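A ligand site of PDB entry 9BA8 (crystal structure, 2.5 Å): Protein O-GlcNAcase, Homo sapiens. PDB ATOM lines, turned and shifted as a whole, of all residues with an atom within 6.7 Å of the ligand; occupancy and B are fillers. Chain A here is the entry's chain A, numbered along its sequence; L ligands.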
ATOM      1  N   GLY A  15       9.259  -0.229   1.710  1.00  0.00           N
ATOM      2  CA  GLY A  15       9.078   1.125   1.194  1.00  0.00           C
ATOM      3  C   GLY A  15       7.773   1.413   0.495  1.00  0.00           C
ATOM      4  O   GLY A  15       7.732   2.240  -0.398  1.00  0.00           O
ATOM      5  N   PHE A  16       6.692   0.778   0.923  1.00  0.00           N
ATOM      6  CA  PHE A  16       5.376   0.942   0.319  1.00  0.00           C
ATOM      7  C   PHE A  16       4.463   1.737   1.205  1.00  0.00           C
ATOM      8  O   PHE A  16       4.806   2.036   2.356  1.00  0.00           O
ATOM      9  CB  PHE A  16       4.756  -0.462   0.085  1.00  0.00           C
ATOM     10  CG  PHE A  16       4.920  -1.411   1.268  1.00  0.00           C
ATOM     11  CD1 PHE A  16       5.895  -2.405   1.254  1.00  0.00           C
ATOM     12  CD2 PHE A  16       4.096  -1.299   2.394  1.00  0.00           C
ATOM     13  CE1 PHE A  16       6.070  -3.259   2.353  1.00  0.00           C
ATOM     14  CE2 PHE A  16       4.265  -2.166   3.490  1.00  0.00           C
ATOM     15  CZ  PHE A  16       5.245  -3.136   3.452  1.00  0.00           C
ATOM     16  N   TYR A  17       3.281   2.053   0.680  1.00  0.00           N
ATOM     17  CA  TYR A  17       2.138   2.641   1.388  1.00  0.00           C
ATOM     18  C   TYR A  17       1.345   1.415   1.854  1.00  0.00           C
ATOM     19  O   TYR A  17       1.242   0.421   1.133  1.00  0.00           O
ATOM     20  CB  TYR A  17       1.248   3.445   0.415  1.00  0.00           C
ATOM     21  CG  TYR A  17       1.913   4.699  -0.098  1.00  0.00           C
ATOM     22  CD1 TYR A  17       1.906   5.860   0.658  1.00  0.00           C
ATOM     23  CD2 TYR A  17       2.562   4.708  -1.331  1.00  0.00           C
ATOM     24  CE1 TYR A  17       2.532   7.014   0.206  1.00  0.00           C
ATOM     25  CE2 TYR A  17       3.187   5.868  -1.801  1.00  0.00           C
ATOM     26  CZ  TYR A  17       3.154   7.011  -1.030  1.00  0.00           C
ATOM     27  OH  TYR A  17       3.771   8.153  -1.463  1.00  0.00           O
ATOM     28  N   ALA A  44      11.898   1.937   5.297  1.00  0.00           N
ATOM     29  CA  ALA A  44      11.290   3.115   4.677  1.00  0.00           C
ATOM     30  C   ALA A  44       9.738   3.019   4.610  1.00  0.00           C
ATOM     31  O   ALA A  44       9.164   3.323   3.558  1.00  0.00           O
ATOM     32  CB  ALA A  44      11.880   3.325   3.274  1.00  0.00           C
ATOM     33  N   LYS A  46       6.286   4.092   4.138  1.00  0.00           N
ATOM     34  CA  LYS A  46       5.652   5.378   3.845  1.00  0.00           C
ATOM     35  C   LYS A  46       4.678   5.784   4.967  1.00  0.00           C
ATOM     36  O   LYS A  46       4.563   6.973   5.271  1.00  0.00           O
ATOM     37  CB  LYS A  46       4.895   5.318   2.503  1.00  0.00           C
ATOM     38  CG  LYS A  46       5.726   5.350   1.226  1.00  0.00           C
ATOM     39  CD  LYS A  46       6.250   6.768   0.843  1.00  0.00           C
ATOM     40  CE  LYS A  46       7.035   6.838  -0.472  1.00  0.00           C
ATOM     41  NZ  LYS A  46       8.207   5.880  -0.516  1.00  0.00           N
ATOM     42  N   ASP A 122      11.519  10.802  -3.190  1.00  0.00           N
ATOM     43  CA  ASP A 122      10.553  10.184  -4.071  1.00  0.00           C
ATOM     44  C   ASP A 122       9.117  10.635  -3.768  1.00  0.00           C
ATOM     45  O   ASP A 122       8.727  10.800  -2.604  1.00  0.00           O
ATOM     46  CB  ASP A 122      10.686   8.662  -3.973  1.00  0.00           C
ATOM     47  CG  ASP A 122      10.390   8.063  -2.598  1.00  0.00           C
ATOM     48  OD1 ASP A 122       9.769   6.994  -2.542  1.00  0.00           O
ATOM     49  OD2 ASP A 122      10.796   8.671  -1.563  1.00  0.00           O
ATOM     50  N   ASP A 123       8.355  10.874  -4.854  1.00  0.00           N
ATOM     51  CA  ASP A 123       6.926  11.188  -4.888  1.00  0.00           C
ATOM     52  C   ASP A 123       6.592  12.507  -4.186  1.00  0.00           C
ATOM     53  O   ASP A 123       5.679  12.615  -3.343  1.00  0.00           O
ATOM     54  CB  ASP A 123       6.107   9.983  -4.360  1.00  0.00           C
ATOM     55  CG  ASP A 123       6.313   8.713  -5.197  1.00  0.00           C
ATOM     56  OD1 ASP A 123       6.247   7.605  -4.621  1.00  0.00           O
ATOM     57  OD2 ASP A 123       6.548   8.840  -6.429  1.00  0.00           O
ATOM     58  N   CYS A 163      17.577   8.907  -2.579  1.00  0.00           N
ATOM     59  CA  CYS A 163      16.597   8.550  -3.578  1.00  0.00           C
ATOM     60  C   CYS A 163      16.165   9.800  -4.288  1.00  0.00           C
ATOM     61  O   CYS A 163      15.652  10.744  -3.658  1.00  0.00           O
ATOM     62  CB  CYS A 163      15.407   7.762  -3.040  1.00  0.00           C
ATOM     63  SG  CYS A 163      14.214   7.333  -4.330  1.00  0.00           S
ATOM     64  N   PRO A 164      16.406   9.838  -5.617  1.00  0.00           N
ATOM     65  CA  PRO A 164      16.059  11.050  -6.367  1.00  0.00           C
ATOM     66  C   PRO A 164      14.576  11.167  -6.628  1.00  0.00           C
ATOM     67  O   PRO A 164      13.858  10.165  -6.564  1.00  0.00           O
ATOM     68  CB  PRO A 164      16.877  10.917  -7.660  1.00  0.00           C
ATOM     69  CG  PRO A 164      17.125   9.442  -7.818  1.00  0.00           C
ATOM     70  CD  PRO A 164      17.046   8.808  -6.477  1.00  0.00           C
ATOM     71  N   TYR A 167      13.542   9.107 -10.168  1.00  0.00           N
ATOM     72  CA  TYR A 167      14.087   7.800  -9.781  1.00  0.00           C
ATOM     73  C   TYR A 167      13.883   6.680 -10.787  1.00  0.00           C
ATOM     74  O   TYR A 167      14.329   5.557 -10.543  1.00  0.00           O
ATOM     75  CB  TYR A 167      13.545   7.391  -8.410  1.00  0.00           C
ATOM     76  CG  TYR A 167      12.038   7.274  -8.306  1.00  0.00           C
ATOM     77  CD1 TYR A 167      11.378   6.124  -8.702  1.00  0.00           C
ATOM     78  CD2 TYR A 167      11.293   8.271  -7.676  1.00  0.00           C
ATOM     79  CE1 TYR A 167      10.015   5.956  -8.497  1.00  0.00           C
ATOM     80  CE2 TYR A 167       9.923   8.117  -7.455  1.00  0.00           C
ATOM     81  CZ  TYR A 167       9.294   6.946  -7.850  1.00  0.00           C
ATOM     82  OH  TYR A 167       7.944   6.776  -7.656  1.00  0.00           O
ATOM     83  N   LEU A 196      19.466   5.563  -5.576  1.00  0.00           N
ATOM     84  CA  LEU A 196      18.447   4.540  -5.802  1.00  0.00           C
ATOM     85  C   LEU A 196      17.745   4.778  -7.146  1.00  0.00           C
ATOM     86  O   LEU A 196      17.615   5.925  -7.580  1.00  0.00           O
ATOM     87  CB  LEU A 196      17.459   4.413  -4.624  1.00  0.00           C
ATOM     88  CG  LEU A 196      18.061   3.931  -3.287  1.00  0.00           C
ATOM     89  CD1 LEU A 196      17.366   4.583  -2.092  1.00  0.00           C
ATOM     90  CD2 LEU A 196      18.099   2.423  -3.190  1.00  0.00           C
ATOM     91  N   TRP A 197      17.377   3.681  -7.837  1.00  0.00           N
ATOM     92  CA  TRP A 197      16.806   3.748  -9.186  1.00  0.00           C
ATOM     93  C   TRP A 197      15.869   2.560  -9.400  1.00  0.00           C
ATOM     94  O   TRP A 197      16.212   1.445  -9.030  1.00  0.00           O
ATOM     95  CB  TRP A 197      17.984   3.756 -10.214  1.00  0.00           C
ATOM     96  CG  TRP A 197      17.589   3.891 -11.644  1.00  0.00           C
ATOM     97  CD1 TRP A 197      17.596   2.898 -12.594  1.00  0.00           C
ATOM     98  CD2 TRP A 197      17.179   5.085 -12.333  1.00  0.00           C
ATOM     99  NE1 TRP A 197      17.236   3.406 -13.818  1.00  0.00           N
ATOM    100  CE2 TRP A 197      16.943   4.740 -13.687  1.00  0.00           C
ATOM    101  CE3 TRP A 197      16.996   6.430 -11.938  1.00  0.00           C
ATOM    102  CZ2 TRP A 197      16.480   5.665 -14.629  1.00  0.00           C
ATOM    103  CZ3 TRP A 197      16.542   7.359 -12.879  1.00  0.00           C
ATOM    104  CH2 TRP A 197      16.311   6.975 -14.216  1.00  0.00           C
ATOM    105  N   THR A 198      14.688   2.807  -9.960  1.00  0.00           N
ATOM    106  CA  THR A 198      13.728   1.716 -10.149  1.00  0.00           C
ATOM    107  C   THR A 198      13.693   1.135 -11.588  1.00  0.00           C
ATOM    108  O   THR A 198      12.866   0.263 -11.876  1.00  0.00           O
ATOM    109  CB  THR A 198      12.311   2.131  -9.669  1.00  0.00           C
ATOM    110  OG1 THR A 198      11.720   3.000 -10.624  1.00  0.00           O
ATOM    111  CG2 THR A 198      12.312   2.756  -8.297  1.00  0.00           C
ATOM    112  N   VAL A 202       8.386   3.034 -12.707  1.00  0.00           N
ATOM    113  CA  VAL A 202       8.226   2.836 -11.259  1.00  0.00           C
ATOM    114  C   VAL A 202       8.177   1.326 -11.051  1.00  0.00           C
ATOM    115  O   VAL A 202       8.925   0.805 -10.225  1.00  0.00           O
ATOM    116  CB  VAL A 202       6.978   3.568 -10.685  1.00  0.00           C
ATOM    117  CG1 VAL A 202       6.809   3.279  -9.195  1.00  0.00           C
ATOM    118  CG2 VAL A 202       7.055   5.074 -10.938  1.00  0.00           C
ATOM    119  N   VAL A 203       7.363   0.618 -11.845  1.00  0.00           N
ATOM    120  CA  VAL A 203       7.278  -0.841 -11.819  1.00  0.00           C
ATOM    121  C   VAL A 203       7.830  -1.256 -13.167  1.00  0.00           C
ATOM    122  O   VAL A 203       7.137  -1.140 -14.183  1.00  0.00           O
ATOM    123  CB  VAL A 203       5.832  -1.374 -11.591  1.00  0.00           C
ATOM    124  CG1 VAL A 203       5.815  -2.900 -11.519  1.00  0.00           C
ATOM    125  CG2 VAL A 203       5.220  -0.773 -10.344  1.00  0.00           C
ATOM    126  N   TRP A 226      16.080  -0.048  -6.494  1.00  0.00           N
ATOM    127  CA  TRP A 226      14.942  -0.116  -5.595  1.00  0.00           C
ATOM    128  C   TRP A 226      13.944  -0.761  -6.569  1.00  0.00           C
ATOM    129  O   TRP A 226      13.470  -0.110  -7.513  1.00  0.00           O
ATOM    130  CB  TRP A 226      14.464   1.292  -5.152  1.00  0.00           C
ATOM    131  CG  TRP A 226      13.138   1.323  -4.442  1.00  0.00           C
ATOM    132  CD1 TRP A 226      11.964   0.749  -4.870  1.00  0.00           C
ATOM    133  CD2 TRP A 226      12.807   2.073  -3.262  1.00  0.00           C
ATOM    134  NE1 TRP A 226      10.936   1.089  -4.012  1.00  0.00           N
ATOM    135  CE2 TRP A 226      11.420   1.904  -3.024  1.00  0.00           C
ATOM    136  CE3 TRP A 226      13.529   2.958  -2.433  1.00  0.00           C
ATOM    137  CZ2 TRP A 226      10.760   2.532  -1.967  1.00  0.00           C
ATOM    138  CZ3 TRP A 226      12.860   3.585  -1.386  1.00  0.00           C
ATOM    139  CH2 TRP A 226      11.498   3.330  -1.137  1.00  0.00           C
ATOM    140  N   ASN A 228      10.493  -2.480  -7.805  1.00  0.00           N
ATOM    141  CA  ASN A 228       9.072  -2.510  -7.515  1.00  0.00           C
ATOM    142  C   ASN A 228       8.327  -3.637  -8.260  1.00  0.00           C
ATOM    143  O   ASN A 228       7.100  -3.628  -8.318  1.00  0.00           O
ATOM    144  CB  ASN A 228       8.425  -1.133  -7.754  1.00  0.00           C
ATOM    145  CG  ASN A 228       8.924  -0.037  -6.836  1.00  0.00           C
ATOM    146  OD1 ASN A 228       8.841  -0.135  -5.612  1.00  0.00           O
ATOM    147  ND2 ASN A 228       9.409   1.043  -7.423  1.00  0.00           N
ATOM    148  N   ALA A 231       5.772  -5.184  -5.825  1.00  0.00           N
ATOM    149  CA  ALA A 231       5.027  -4.192  -5.058  1.00  0.00           C
ATOM    150  C   ALA A 231       3.504  -4.244  -5.388  1.00  0.00           C
ATOM    151  O   ALA A 231       3.135  -4.512  -6.527  1.00  0.00           O
ATOM    152  CB  ALA A 231       5.578  -2.808  -5.348  1.00  0.00           C
ATOM    153  N   ASN A 232       2.616  -4.003  -4.403  1.00  0.00           N
ATOM    154  CA  ASN A 232       1.187  -4.072  -4.723  1.00  0.00           C
ATOM    155  C   ASN A 232       0.342  -2.989  -4.014  1.00  0.00           C
ATOM    156  O   ASN A 232      -0.850  -3.179  -3.783  1.00  0.00           O
ATOM    157  CB  ASN A 232       0.647  -5.479  -4.451  1.00  0.00           C
ATOM    158  CG  ASN A 232       0.717  -5.920  -3.029  1.00  0.00           C
ATOM    159  OD1 ASN A 232       1.391  -5.326  -2.204  1.00  0.00           O
ATOM    160  ND2 ASN A 232       0.032  -6.984  -2.702  1.00  0.00           N
ATOM    161  N   ASP A 233       0.942  -1.857  -3.706  1.00  0.00           N
ATOM    162  CA  ASP A 233       0.180  -0.838  -3.002  1.00  0.00           C
ATOM    163  C   ASP A 233      -0.619   0.049  -3.929  1.00  0.00           C
ATOM    164  O   ASP A 233      -1.392   0.905  -3.486  1.00  0.00           O
ATOM    165  CB  ASP A 233       1.070  -0.016  -2.045  1.00  0.00           C
ATOM    166  CG  ASP A 233       2.231   0.712  -2.677  1.00  0.00           C
ATOM    167  OD1 ASP A 233       2.780   1.606  -2.026  1.00  0.00           O
ATOM    168  OD2 ASP A 233       2.632   0.334  -3.790  1.00  0.00           O
ATOM    169  N   TYR A 234      -0.490  -0.166  -5.225  1.00  0.00           N
ATOM    170  CA  TYR A 234      -1.228   0.661  -6.165  1.00  0.00           C
ATOM    171  C   TYR A 234      -2.550   0.003  -6.499  1.00  0.00           C
ATOM    172  O   TYR A 234      -3.466   0.674  -6.975  1.00  0.00           O
ATOM    173  CB  TYR A 234      -0.374   0.975  -7.386  1.00  0.00           C
ATOM    174  CG  TYR A 234       0.200  -0.242  -8.086  1.00  0.00           C
ATOM    175  CD1 TYR A 234      -0.450  -0.804  -9.176  1.00  0.00           C
ATOM    176  CD2 TYR A 234       1.448  -0.743  -7.726  1.00  0.00           C
ATOM    177  CE1 TYR A 234       0.097  -1.891  -9.849  1.00  0.00           C
ATOM    178  CE2 TYR A 234       2.013  -1.816  -8.416  1.00  0.00           C
ATOM    179  CZ  TYR A 234       1.328  -2.380  -9.484  1.00  0.00           C
ATOM    180  OH  TYR A 234       1.873  -3.426 -10.207  1.00  0.00           O
ATOM    181  N   ASP A 235      -2.689  -1.283  -6.164  1.00  0.00           N
ATOM    182  CA  ASP A 235      -3.950  -1.960  -6.370  1.00  0.00           C
ATOM    183  C   ASP A 235      -4.312  -2.875  -5.231  1.00  0.00           C
ATOM    184  O   ASP A 235      -3.597  -3.839  -4.976  1.00  0.00           O
ATOM    185  CB  ASP A 235      -4.028  -2.689  -7.721  1.00  0.00           C
ATOM    186  CG  ASP A 235      -5.447  -2.949  -8.173  1.00  0.00           C
ATOM    187  OD1 ASP A 235      -6.237  -3.532  -7.392  1.00  0.00           O
ATOM    188  OD2 ASP A 235      -5.764  -2.630  -9.339  1.00  0.00           O
ATOM    189  N   ASN A 261      11.227  -4.014  -3.161  1.00  0.00           N
ATOM    190  CA  ASN A 261      10.082  -3.391  -2.483  1.00  0.00           C
ATOM    191  C   ASN A 261       8.923  -4.309  -2.759  1.00  0.00           C
ATOM    192  O   ASN A 261       8.343  -4.212  -3.830  1.00  0.00           O
ATOM    193  CB  ASN A 261       9.808  -1.973  -3.004  1.00  0.00           C
ATOM    194  CG  ASN A 261       8.802  -1.198  -2.183  1.00  0.00           C
ATOM    195  OD1 ASN A 261       8.648  -1.406  -0.973  1.00  0.00           O
ATOM    196  ND2 ASN A 261       8.092  -0.282  -2.828  1.00  0.00           N
HETATM  197  O1  LIG L   1       1.354   3.752  -7.359  1.00  0.00           O
HETATM  198  C1  LIG L   1       5.079   0.684  -6.881  1.00  0.00           C
HETATM  199  O2  LIG L   1      -1.800   4.168 -10.155  1.00  0.00           O
HETATM  200  C2  LIG L   1       4.641   2.071  -6.426  1.00  0.00           C
HETATM  201  C3  LIG L   1      11.705   5.174  -5.264  1.00  0.00           C
HETATM  202  N1  LIG L   1       7.651   4.468  -2.947  1.00  0.00           N
HETATM  203  C4  LIG L   1       5.397   1.681  -4.001  1.00  0.00           C
HETATM  204  C5  LIG L   1       6.422   2.673  -3.809  1.00  0.00           C
HETATM  205  C6  LIG L   1       6.532   3.669  -2.842  1.00  0.00           C
HETATM  206  C7  LIG L   1       8.367   4.131  -3.988  1.00  0.00           C
HETATM  207  F1  LIG L   1       5.681   3.927  -1.853  1.00  0.00           F
HETATM  208  S1  LIG L   1       7.778   2.788  -4.893  1.00  0.00           S
HETATM  209  N2  LIG L   1       9.542   4.799  -4.292  1.00  0.00           N
HETATM  210  C8  LIG L   1      10.368   4.510  -5.322  1.00  0.00           C
HETATM  211  O3  LIG L   1      10.062   3.740  -6.208  1.00  0.00           O
HETATM  212  N3  LIG L   1       4.304   2.093  -4.943  1.00  0.00           N
HETATM  213  C9  LIG L   1       3.766   3.451  -4.567  1.00  0.00           C
HETATM  214  C10 LIG L   1       2.428   3.662  -5.260  1.00  0.00           C
HETATM  215  C11 LIG L   1       2.641   3.679  -6.753  1.00  0.00           C
HETATM  216  C12 LIG L   1       3.353   2.420  -7.231  1.00  0.00           C
HETATM  217  C13 LIG L   1       1.194   4.811  -8.302  1.00  0.00           C
HETATM  218  C14 LIG L   1      -0.159   4.574  -8.855  1.00  0.00           C
HETATM  219  N4  LIG L   1      -0.390   4.319 -10.103  1.00  0.00           N
HETATM  220  C15 LIG L   1      -2.233   4.358  -8.895  1.00  0.00           C
HETATM  221  N5  LIG L   1      -1.274   4.604  -8.061  1.00  0.00           N
HETATM  222  C16 LIG L   1      -3.686   4.239  -8.656  1.00  0.00           C
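The backbone carbonyl oxygen of Gly 15 lies close to a fluorine (F1) of the ligand (3.0 Å). Merely in contact with the ligand: Phe 16 (3.7 Å), Tyr 17 (3.2 Å), Asp 123 (3.8 Å), Cys 163 (3.4 Å), Tyr 167 (3.2 Å), Thr 198 (3.2 Å), Val 202 (3.7 Å), Val 203 (3.8 Å), Ala 231 (3.8 Å) and Tyr 234 (3.3 Å). Hydrophobic or aromatic side chains within 4 Å of the ligand: Tyr 17, Tyr 167, Val 202, Val 203, Trp 226, Ala 231 and Tyr 234. The nearest printed residue that does not touch the ligand is Pro 164 (5.6 Å).
NZ of Lys 46 lies within salt-bridge range of OD1 of Asp 122. The side-chain amide nitrogen of Asn 261 lies within hydrogen-bond range of the side-chain amide oxygen of Asn 228, 2.9 Å away. The backbone NH (N) of Thr 198 lies within hydrogen-bond range of the backbone carbonyl oxygen (O) of Tyr 167, 2.8 Å away. OH of Tyr 167 sits at hydrogen-bond distance from OD2 of Asp 123. The side-chain amide nitrogen (ND2) of Asn 261 lies close to the indole nitrogen (NE1) of Trp 226, at 3.4 Å. The backbone carbonyl oxygen (O) of Trp 197 lies within hydrogen-bond range of the backbone NH (N) of Trp 226 (2.9 Å). The side-chain amide oxygen of Asn 261 lies within hydrogen-bond range of the backbone NH of Phe 16. O of Asn 261 lies within hydrogen-bond range of N of Ala 231, 3.4 Å away.
N3 of the ligand lies within salt-bridge range of OD2 of Asp 233, 2.7 Å away. OD1 of Asp 122 is in hydrogen-bond range of N2 of the ligand (2.8 Å). The side-chain amino group (NZ) of Lys 46 lies within hydrogen-bond range of a nitrogen (N1) of the ligand, at 2.9 Å. The side-chain amide nitrogen of Asn 228 is in hydrogen-bond range of an oxygen (O3) of the ligand (3.0 Å). The indole nitrogen (NE1) of Trp 226 lies close to a sulfur (S1) of the ligand. The side-chain amide nitrogen (ND2) of Asn 261 lies close to a sulfur (S1) of the ligand (3.7 Å).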
